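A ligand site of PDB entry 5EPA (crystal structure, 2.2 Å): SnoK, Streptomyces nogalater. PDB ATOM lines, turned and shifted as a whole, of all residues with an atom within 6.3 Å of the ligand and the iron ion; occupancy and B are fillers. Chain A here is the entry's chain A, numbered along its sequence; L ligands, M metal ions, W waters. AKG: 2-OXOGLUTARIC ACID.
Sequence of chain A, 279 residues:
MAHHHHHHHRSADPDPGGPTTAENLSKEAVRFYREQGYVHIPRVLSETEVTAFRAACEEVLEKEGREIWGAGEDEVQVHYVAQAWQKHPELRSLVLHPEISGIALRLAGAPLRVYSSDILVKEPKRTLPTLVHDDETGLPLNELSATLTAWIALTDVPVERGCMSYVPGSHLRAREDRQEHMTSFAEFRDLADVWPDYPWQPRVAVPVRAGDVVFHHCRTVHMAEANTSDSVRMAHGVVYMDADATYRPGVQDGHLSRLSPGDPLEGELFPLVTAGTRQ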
ATOM      1  N   TRP A  69      16.203  13.702  -9.198  1.00  0.00           N
ATOM      2  CA  TRP A  69      15.638  13.408 -10.489  1.00  0.00           C
ATOM      3  C   TRP A  69      14.987  12.056 -10.325  1.00  0.00           C
ATOM      4  O   TRP A  69      15.667  11.040 -10.156  1.00  0.00           O
ATOM      5  CB  TRP A  69      16.750  13.411 -11.544  1.00  0.00           C
ATOM      6  CG  TRP A  69      16.416  13.035 -12.954  1.00  0.00           C
ATOM      7  CD1 TRP A  69      15.271  12.476 -13.435  1.00  0.00           C
ATOM      8  CD2 TRP A  69      17.333  13.117 -14.072  1.00  0.00           C
ATOM      9  NE1 TRP A  69      15.394  12.228 -14.808  1.00  0.00           N
ATOM     10  CE2 TRP A  69      16.663  12.593 -15.206  1.00  0.00           C
ATOM     11  CE3 TRP A  69      18.654  13.551 -14.202  1.00  0.00           C
ATOM     12  CZ2 TRP A  69      17.262  12.526 -16.473  1.00  0.00           C
ATOM     13  CZ3 TRP A  69      19.268  13.475 -15.456  1.00  0.00           C
ATOM     14  CH2 TRP A  69      18.573  12.961 -16.575  1.00  0.00           C
ATOM     15  N   GLN A  77      16.482   8.349  -9.529  1.00  0.00           N
ATOM     16  CA  GLN A  77      17.362   8.047 -10.669  1.00  0.00           C
ATOM     17  C   GLN A  77      18.721   8.715 -10.522  1.00  0.00           C
ATOM     18  O   GLN A  77      19.741   8.075 -10.713  1.00  0.00           O
ATOM     19  CB  GLN A  77      16.705   8.496 -11.984  1.00  0.00           C
ATOM     20  CG  GLN A  77      15.408   7.776 -12.242  1.00  0.00           C
ATOM     21  CD  GLN A  77      14.674   8.263 -13.484  1.00  0.00           C
ATOM     22  OE1 GLN A  77      15.256   8.593 -14.510  1.00  0.00           O
ATOM     23  NE2 GLN A  77      13.362   8.330 -13.354  1.00  0.00           N
ATOM     24  N   VAL A  78      18.721  10.024 -10.234  1.00  0.00           N
ATOM     25  CA  VAL A  78      19.944  10.798 -10.111  1.00  0.00           C
ATOM     26  C   VAL A  78      19.775  11.884  -9.064  1.00  0.00           C
ATOM     27  O   VAL A  78      18.686  12.467  -8.937  1.00  0.00           O
ATOM     28  CB  VAL A  78      20.296  11.468 -11.442  1.00  0.00           C
ATOM     29  CG1 VAL A  78      21.609  12.186 -11.335  1.00  0.00           C
ATOM     30  CG2 VAL A  78      20.417  10.457 -12.562  1.00  0.00           C
ATOM     31  N   LEU A 120      25.865  15.351 -11.433  1.00  0.00           N
ATOM     32  CA  LEU A 120      25.015  14.145 -11.677  1.00  0.00           C
ATOM     33  C   LEU A 120      25.535  12.928 -10.920  1.00  0.00           C
ATOM     34  O   LEU A 120      26.485  12.260 -11.338  1.00  0.00           O
ATOM     35  CB  LEU A 120      24.954  13.827 -13.160  1.00  0.00           C
ATOM     36  CG  LEU A 120      24.363  14.915 -14.066  1.00  0.00           C
ATOM     37  CD1 LEU A 120      24.854  14.660 -15.487  1.00  0.00           C
ATOM     38  CD2 LEU A 120      22.849  14.989 -13.987  1.00  0.00           C
ATOM     39  N   VAL A 121      24.902  12.667  -9.778  1.00  0.00           N
ATOM     40  CA  VAL A 121      25.415  11.676  -8.804  1.00  0.00           C
ATOM     41  C   VAL A 121      24.486  10.497  -8.728  1.00  0.00           C
ATOM     42  O   VAL A 121      23.259  10.678  -8.690  1.00  0.00           O
ATOM     43  CB  VAL A 121      25.540  12.292  -7.390  1.00  0.00           C
ATOM     44  CG1 VAL A 121      25.689  11.231  -6.325  1.00  0.00           C
ATOM     45  CG2 VAL A 121      26.743  13.208  -7.327  1.00  0.00           C
ATOM     46  N   LYS A 122      25.045   9.290  -8.722  1.00  0.00           N
ATOM     47  CA  LYS A 122      24.259   8.080  -8.419  1.00  0.00           C
ATOM     48  C   LYS A 122      24.847   7.358  -7.211  1.00  0.00           C
ATOM     49  O   LYS A 122      25.967   6.892  -7.288  1.00  0.00           O
ATOM     50  CB  LYS A 122      24.179   7.098  -9.614  1.00  0.00           C
ATOM     51  CG  LYS A 122      23.194   7.497 -10.723  1.00  0.00           C
ATOM     52  CD  LYS A 122      23.087   6.361 -11.763  1.00  0.00           C
ATOM     53  CE  LYS A 122      22.212   6.716 -12.973  1.00  0.00           C
ATOM     54  NZ  LYS A 122      20.778   6.442 -12.727  1.00  0.00           N
ATOM     55  N   THR A 130      18.512   5.623 -15.069  1.00  0.00           N
ATOM     56  CA  THR A 130      18.039   6.886 -15.628  1.00  0.00           C
ATOM     57  C   THR A 130      17.209   6.561 -16.881  1.00  0.00           C
ATOM     58  O   THR A 130      17.716   6.024 -17.861  1.00  0.00           O
ATOM     59  CB  THR A 130      19.174   7.808 -16.013  1.00  0.00           C
ATOM     60  OG1 THR A 130      20.029   8.029 -14.884  1.00  0.00           O
ATOM     61  CG2 THR A 130      18.622   9.132 -16.474  1.00  0.00           C
ATOM     62  N   HIS A 133      15.720   8.856 -22.800  1.00  0.00           N
ATOM     63  CA  HIS A 133      15.210  10.130 -23.316  1.00  0.00           C
ATOM     64  C   HIS A 133      16.159  10.713 -24.324  1.00  0.00           C
ATOM     65  O   HIS A 133      17.260  10.197 -24.504  1.00  0.00           O
ATOM     66  CB  HIS A 133      15.029  11.146 -22.159  1.00  0.00           C
ATOM     67  CG  HIS A 133      16.321  11.508 -21.456  1.00  0.00           C
ATOM     68  ND1 HIS A 133      16.944  10.666 -20.563  1.00  0.00           N
ATOM     69  CD2 HIS A 133      17.110  12.613 -21.553  1.00  0.00           C
ATOM     70  CE1 HIS A 133      18.068  11.243 -20.136  1.00  0.00           C
ATOM     71  NE2 HIS A 133      18.223  12.410 -20.758  1.00  0.00           N
ATOM     72  N   ASP A 134      15.755  11.791 -24.972  1.00  0.00           N
ATOM     73  CA  ASP A 134      16.712  12.677 -25.619  1.00  0.00           C
ATOM     74  C   ASP A 134      16.663  14.014 -24.879  1.00  0.00           C
ATOM     75  O   ASP A 134      15.764  14.255 -24.086  1.00  0.00           O
ATOM     76  CB  ASP A 134      16.468  12.863 -27.100  1.00  0.00           C
ATOM     77  CG  ASP A 134      15.134  13.574 -27.444  1.00  0.00           C
ATOM     78  OD1 ASP A 134      14.745  14.544 -26.757  1.00  0.00           O
ATOM     79  OD2 ASP A 134      14.498  13.150 -28.442  1.00  0.00           O
ATOM     80  N   ASP A 135      17.685  14.827 -25.052  1.00  0.00           N
ATOM     81  CA  ASP A 135      17.827  16.032 -24.204  1.00  0.00           C
ATOM     82  C   ASP A 135      17.004  17.167 -24.770  1.00  0.00           C
ATOM     83  O   ASP A 135      16.472  17.975 -24.031  1.00  0.00           O
ATOM     84  CB  ASP A 135      19.280  16.413 -24.078  1.00  0.00           C
ATOM     85  CG  ASP A 135      20.083  15.447 -23.213  1.00  0.00           C
ATOM     86  OD1 ASP A 135      19.585  14.785 -22.228  1.00  0.00           O
ATOM     87  OD2 ASP A 135      21.282  15.362 -23.548  1.00  0.00           O
ATOM     88  N   THR A 149      25.899  17.645 -25.422  1.00  0.00           N
ATOM     89  CA  THR A 149      26.226  17.551 -24.008  1.00  0.00           C
ATOM     90  C   THR A 149      27.550  16.838 -23.828  1.00  0.00           C
ATOM     91  O   THR A 149      27.808  15.838 -24.516  1.00  0.00           O
ATOM     92  CB  THR A 149      25.177  16.752 -23.244  1.00  0.00           C
ATOM     93  OG1 THR A 149      23.896  17.425 -23.258  1.00  0.00           O
ATOM     94  CG2 THR A 149      25.599  16.513 -21.799  1.00  0.00           C
ATOM     95  N   ALA A 150      28.393  17.383 -22.964  1.00  0.00           N
ATOM     96  CA  ALA A 150      29.607  16.728 -22.520  1.00  0.00           C
ATOM     97  C   ALA A 150      29.330  16.089 -21.165  1.00  0.00           C
ATOM     98  O   ALA A 150      29.030  16.774 -20.209  1.00  0.00           O
ATOM     99  CB  ALA A 150      30.727  17.745 -22.371  1.00  0.00           C
ATOM    100  N   TRP A 151      29.430  14.773 -21.089  1.00  0.00           N
ATOM    101  CA  TRP A 151      29.204  14.029 -19.845  1.00  0.00           C
ATOM    102  C   TRP A 151      30.548  13.650 -19.328  1.00  0.00           C
ATOM    103  O   TRP A 151      31.217  12.775 -19.880  1.00  0.00           O
ATOM    104  CB  TRP A 151      28.355  12.814 -20.142  1.00  0.00           C
ATOM    105  CG  TRP A 151      27.746  12.111 -18.945  1.00  0.00           C
ATOM    106  CD1 TRP A 151      26.570  12.381 -18.341  1.00  0.00           C
ATOM    107  CD2 TRP A 151      28.280  10.959 -18.290  1.00  0.00           C
ATOM    108  NE1 TRP A 151      26.342  11.492 -17.317  1.00  0.00           N
ATOM    109  CE2 TRP A 151      27.392  10.607 -17.278  1.00  0.00           C
ATOM    110  CE3 TRP A 151      29.459  10.218 -18.452  1.00  0.00           C
ATOM    111  CZ2 TRP A 151      27.595   9.512 -16.456  1.00  0.00           C
ATOM    112  CZ3 TRP A 151      29.689   9.145 -17.591  1.00  0.00           C
ATOM    113  CH2 TRP A 151      28.769   8.812 -16.605  1.00  0.00           C
ATOM    114  N   GLY A 162      26.584   2.661 -12.931  1.00  0.00           N
ATOM    115  CA  GLY A 162      25.655   3.623 -13.513  1.00  0.00           C
ATOM    116  C   GLY A 162      26.112   4.283 -14.794  1.00  0.00           C
ATOM    117  O   GLY A 162      25.966   5.491 -14.981  1.00  0.00           O
ATOM    118  N   MET A 164      26.477   5.252 -18.874  1.00  0.00           N
ATOM    119  CA  MET A 164      25.529   5.691 -19.892  1.00  0.00           C
ATOM    120  C   MET A 164      25.414   4.649 -21.011  1.00  0.00           C
ATOM    121  O   MET A 164      26.365   3.938 -21.261  1.00  0.00           O
ATOM    122  CB  MET A 164      26.008   6.997 -20.517  1.00  0.00           C
ATOM    123  CG  MET A 164      26.153   8.145 -19.521  1.00  0.00           C
ATOM    124  SD  MET A 164      24.560   8.863 -19.155  1.00  0.00           S
ATOM    125  CE  MET A 164      24.377   9.871 -20.604  1.00  0.00           C
ATOM    126  N   HIS A 216      27.364  13.689 -26.419  1.00  0.00           N
ATOM    127  CA  HIS A 216      26.200  13.225 -27.200  1.00  0.00           C
ATOM    128  C   HIS A 216      25.317  14.375 -27.675  1.00  0.00           C
ATOM    129  O   HIS A 216      25.032  15.326 -26.943  1.00  0.00           O
ATOM    130  CB  HIS A 216      25.369  12.128 -26.414  1.00  0.00           C
ATOM    131  CG  HIS A 216      24.654  12.630 -25.195  1.00  0.00           C
ATOM    132  ND1 HIS A 216      25.235  12.633 -23.957  1.00  0.00           N
ATOM    133  CD2 HIS A 216      23.427  13.193 -25.038  1.00  0.00           C
ATOM    134  CE1 HIS A 216      24.408  13.178 -23.078  1.00  0.00           C
ATOM    135  NE2 HIS A 216      23.289  13.472 -23.702  1.00  0.00           N
ATOM    136  N   HIS A 222      19.395   8.344 -25.213  1.00  0.00           N
ATOM    137  CA  HIS A 222      20.286   7.776 -24.253  1.00  0.00           C
ATOM    138  C   HIS A 222      19.620   7.469 -22.920  1.00  0.00           C
ATOM    139  O   HIS A 222      18.489   7.847 -22.647  1.00  0.00           O
ATOM    140  CB  HIS A 222      21.471   8.730 -24.044  1.00  0.00           C
ATOM    141  CG  HIS A 222      21.074  10.083 -23.509  1.00  0.00           C
ATOM    142  ND1 HIS A 222      20.531  11.059 -24.314  1.00  0.00           N
ATOM    143  CD2 HIS A 222      21.175  10.635 -22.264  1.00  0.00           C
ATOM    144  CE1 HIS A 222      20.291  12.148 -23.585  1.00  0.00           C
ATOM    145  NE2 HIS A 222      20.640  11.918 -22.323  1.00  0.00           N
ATOM    146  N   MET A 223      20.373   6.794 -22.060  1.00  0.00           N
ATOM    147  CA  MET A 223      19.852   6.341 -20.788  1.00  0.00           C
ATOM    148  C   MET A 223      21.047   6.040 -19.862  1.00  0.00           C
ATOM    149  O   MET A 223      22.181   6.157 -20.292  1.00  0.00           O
ATOM    150  CB  MET A 223      18.956   5.114 -21.014  1.00  0.00           C
ATOM    151  CG  MET A 223      19.732   3.841 -21.352  1.00  0.00           C
ATOM    152  SD  MET A 223      18.787   2.728 -22.394  1.00  0.00           S
ATOM    153  CE  MET A 223      19.035   3.518 -23.993  1.00  0.00           C
ATOM    154  N   ALA A 224      20.794   5.627 -18.623  1.00  0.00           N
ATOM    155  CA  ALA A 224      21.865   5.131 -17.754  1.00  0.00           C
ATOM    156  C   ALA A 224      21.443   4.002 -16.855  1.00  0.00           C
ATOM    157  O   ALA A 224      20.319   3.921 -16.457  1.00  0.00           O
ATOM    158  CB  ALA A 224      22.432   6.267 -16.914  1.00  0.00           C
ATOM    159  N   GLU A 225      22.406   3.167 -16.494  1.00  0.00           N
ATOM    160  CA  GLU A 225      22.202   2.057 -15.560  1.00  0.00           C
ATOM    161  C   GLU A 225      21.951   2.544 -14.166  1.00  0.00           C
ATOM    162  O   GLU A 225      22.373   3.624 -13.803  1.00  0.00           O
ATOM    163  CB  GLU A 225      23.463   1.197 -15.421  1.00  0.00           C
ATOM    164  CG  GLU A 225      23.973   0.581 -16.695  1.00  0.00           C
ATOM    165  CD  GLU A 225      22.911  -0.245 -17.361  1.00  0.00           C
ATOM    166  OE1 GLU A 225      22.524  -1.266 -16.764  1.00  0.00           O
ATOM    167  OE2 GLU A 225      22.443   0.150 -18.467  1.00  0.00           O
ATOM    168  N   ARG A 233      28.842   7.134  -7.968  1.00  0.00           N
ATOM    169  CA  ARG A 233      29.184   7.634  -9.314  1.00  0.00           C
ATOM    170  C   ARG A 233      28.975   9.122  -9.401  1.00  0.00           C
ATOM    171  O   ARG A 233      27.897   9.612  -9.053  1.00  0.00           O
ATOM    172  CB  ARG A 233      28.279   7.030 -10.389  1.00  0.00           C
ATOM    173  CG  ARG A 233      28.649   7.484 -11.770  1.00  0.00           C
ATOM    174  CD  ARG A 233      27.472   7.422 -12.716  1.00  0.00           C
ATOM    175  NE  ARG A 233      26.768   8.677 -12.738  1.00  0.00           N
ATOM    176  CZ  ARG A 233      25.682   8.955 -13.442  1.00  0.00           C
ATOM    177  NH1 ARG A 233      25.070   8.058 -14.246  1.00  0.00           N
ATOM    178  NH2 ARG A 233      25.175  10.159 -13.315  1.00  0.00           N
ATOM    179  N   ALA A 235      29.217  12.207 -12.288  1.00  0.00           N
ATOM    180  CA  ALA A 235      29.565  12.887 -13.517  1.00  0.00           C
ATOM    181  C   ALA A 235      29.159  14.366 -13.450  1.00  0.00           C
ATOM    182  O   ALA A 235      28.394  14.776 -12.571  1.00  0.00           O
ATOM    183  CB  ALA A 235      28.892  12.210 -14.707  1.00  0.00           C
ATOM    184  N   GLY A 237      27.535  17.021 -16.224  1.00  0.00           N
ATOM    185  CA  GLY A 237      26.973  17.146 -17.556  1.00  0.00           C
ATOM    186  C   GLY A 237      26.969  18.605 -17.939  1.00  0.00           C
ATOM    187  O   GLY A 237      26.408  19.417 -17.247  1.00  0.00           O
ATOM    188  N   VAL A 238      27.578  18.929 -19.062  1.00  0.00           N
ATOM    189  CA  VAL A 238      27.577  20.311 -19.547  1.00  0.00           C
ATOM    190  C   VAL A 238      26.802  20.408 -20.872  1.00  0.00           C
ATOM    191  O   VAL A 238      27.166  19.744 -21.829  1.00  0.00           O
ATOM    192  CB  VAL A 238      29.007  20.818 -19.788  1.00  0.00           C
ATOM    193  CG1 VAL A 238      28.983  22.281 -20.197  1.00  0.00           C
ATOM    194  CG2 VAL A 238      29.818  20.656 -18.558  1.00  0.00           C
HETATM  195  C1  AKG L   1      22.592  13.625 -19.785  1.00  0.00           C
HETATM  196  O1  AKG L   1      23.774  13.989 -19.528  1.00  0.00           O
HETATM  197  O2  AKG L   1      21.843  14.102 -20.679  1.00  0.00           O
HETATM  198  C2  AKG L   1      21.967  12.596 -18.969  1.00  0.00           C
HETATM  199  O5  AKG L   1      20.831  12.316 -19.306  1.00  0.00           O
HETATM  200  C3  AKG L   1      22.705  11.938 -17.820  1.00  0.00           C
HETATM  201  C4  AKG L   1      21.881  11.021 -16.917  1.00  0.00           C
HETATM  202  C5  AKG L   1      22.792  10.387 -15.845  1.00  0.00           C
HETATM  203  O3  AKG L   1      23.888  10.923 -15.489  1.00  0.00           O
HETATM  204  O4  AKG L   1      22.445   9.328 -15.307  1.00  0.00           O
HETATM  205 FE    FE M   1      20.068  13.439 -20.928  1.00  0.00          FE
HETATM  206  O   HOH W   1      21.576  15.813 -17.747  1.00  0.00           O
HETATM  207  O   HOH W   2      22.002  16.877 -21.155  1.00  0.00           O
HETATM  208  O   HOH W   3      19.419  14.931 -19.507  1.00  0.00           O
HETATM  209  O   HOH W   4      23.731  16.895 -18.854  1.00  0.00           O
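NH2 of Arg 233 is in salt-bridge range of O3 of the ligand, 2.6 Å away.
An oxygen (O4) of the ligand lies within hydrogen-bond range of the side-chain hydroxyl of Thr 130, at 2.8 Å.
NE1 of Trp 151 sits at hydrogen-bond distance from O3 of the ligand (3.1 Å).
NE2 of His 216 lies close to O2 of the ligand (3.4 Å).
Water W2 lies within hydrogen-bond range of the side-chain hydroxyl (OG1) of Thr 149 (2.9 Å) and the side-chain carboxylate (OD2) of Asp 135 (2.9 Å).
OD2 of Asp 135 sits at hydrogen-bond distance from NE2 of His 216 (2.8 Å).
The side-chain carboxylate (OD2) of Asp 135 is in hydrogen-bond range of the side-chain hydroxyl (OG1) of Thr 149 (3.3 Å).
A ring nitrogen (NE2) of His 222 sits close to a ring nitrogen (NE2) of His 216 (3.4 Å).
The backbone carbonyl oxygen (O) of Leu 120 lies within hydrogen-bond range of the guanidinium group (NH2) of Arg 233 (3.2 Å).
The backbone carbonyl oxygen (O) of Ala 224 is in hydrogen-bond range of the backbone NH (N) of Thr 130.
The side-chain hydroxyl (OG1) of Thr 130 sits at hydrogen-bond distance from the side-chain amino group (NZ) of Lys 122 (2.8 Å).
SD of Met 164 is in hydrogen-bond range of NE1 of Trp 151, at 3.7 Å.
The backbone carbonyl oxygen of Val 78 lies within hydrogen-bond range of the backbone NH of Trp 69, at 2.8 Å.
The iron ion is bound by O2 of the ligand, OD1 of Asp 135, O5 of the ligand, NE2 of His 133, NE2 of His 222 and water W3.
CH2 of Trp 69 touches O5 of the ligand, at 3.6 Å.
CG2 of Val 78 touches O4 of the ligand (3.6 Å).
CD1 of Leu 120 touches O3 of the ligand, 3.9 Å away.
Lys 122 touches the ligand.
Thr 149 touches the ligand.
Met 164 touches the ligand.
Ala 224 touches the ligand.
Hydrophobic or aromatic side chains that line the ligand: Trp 69, Val 78, Leu 120, His 133, Trp 151, Met 164, His 216, His 222 and Ala 224.
Within 4 Å of the ligand: Trp 69, Val 78, Leu 120, Lys 122, Thr 130, His 133, Asp 135, Thr 149, Trp 151, Met 164, His 216, His 222, Ala 224 and Arg 233.
Along chain A the residues within 4 Å of the ligand span positions 69 to 233.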
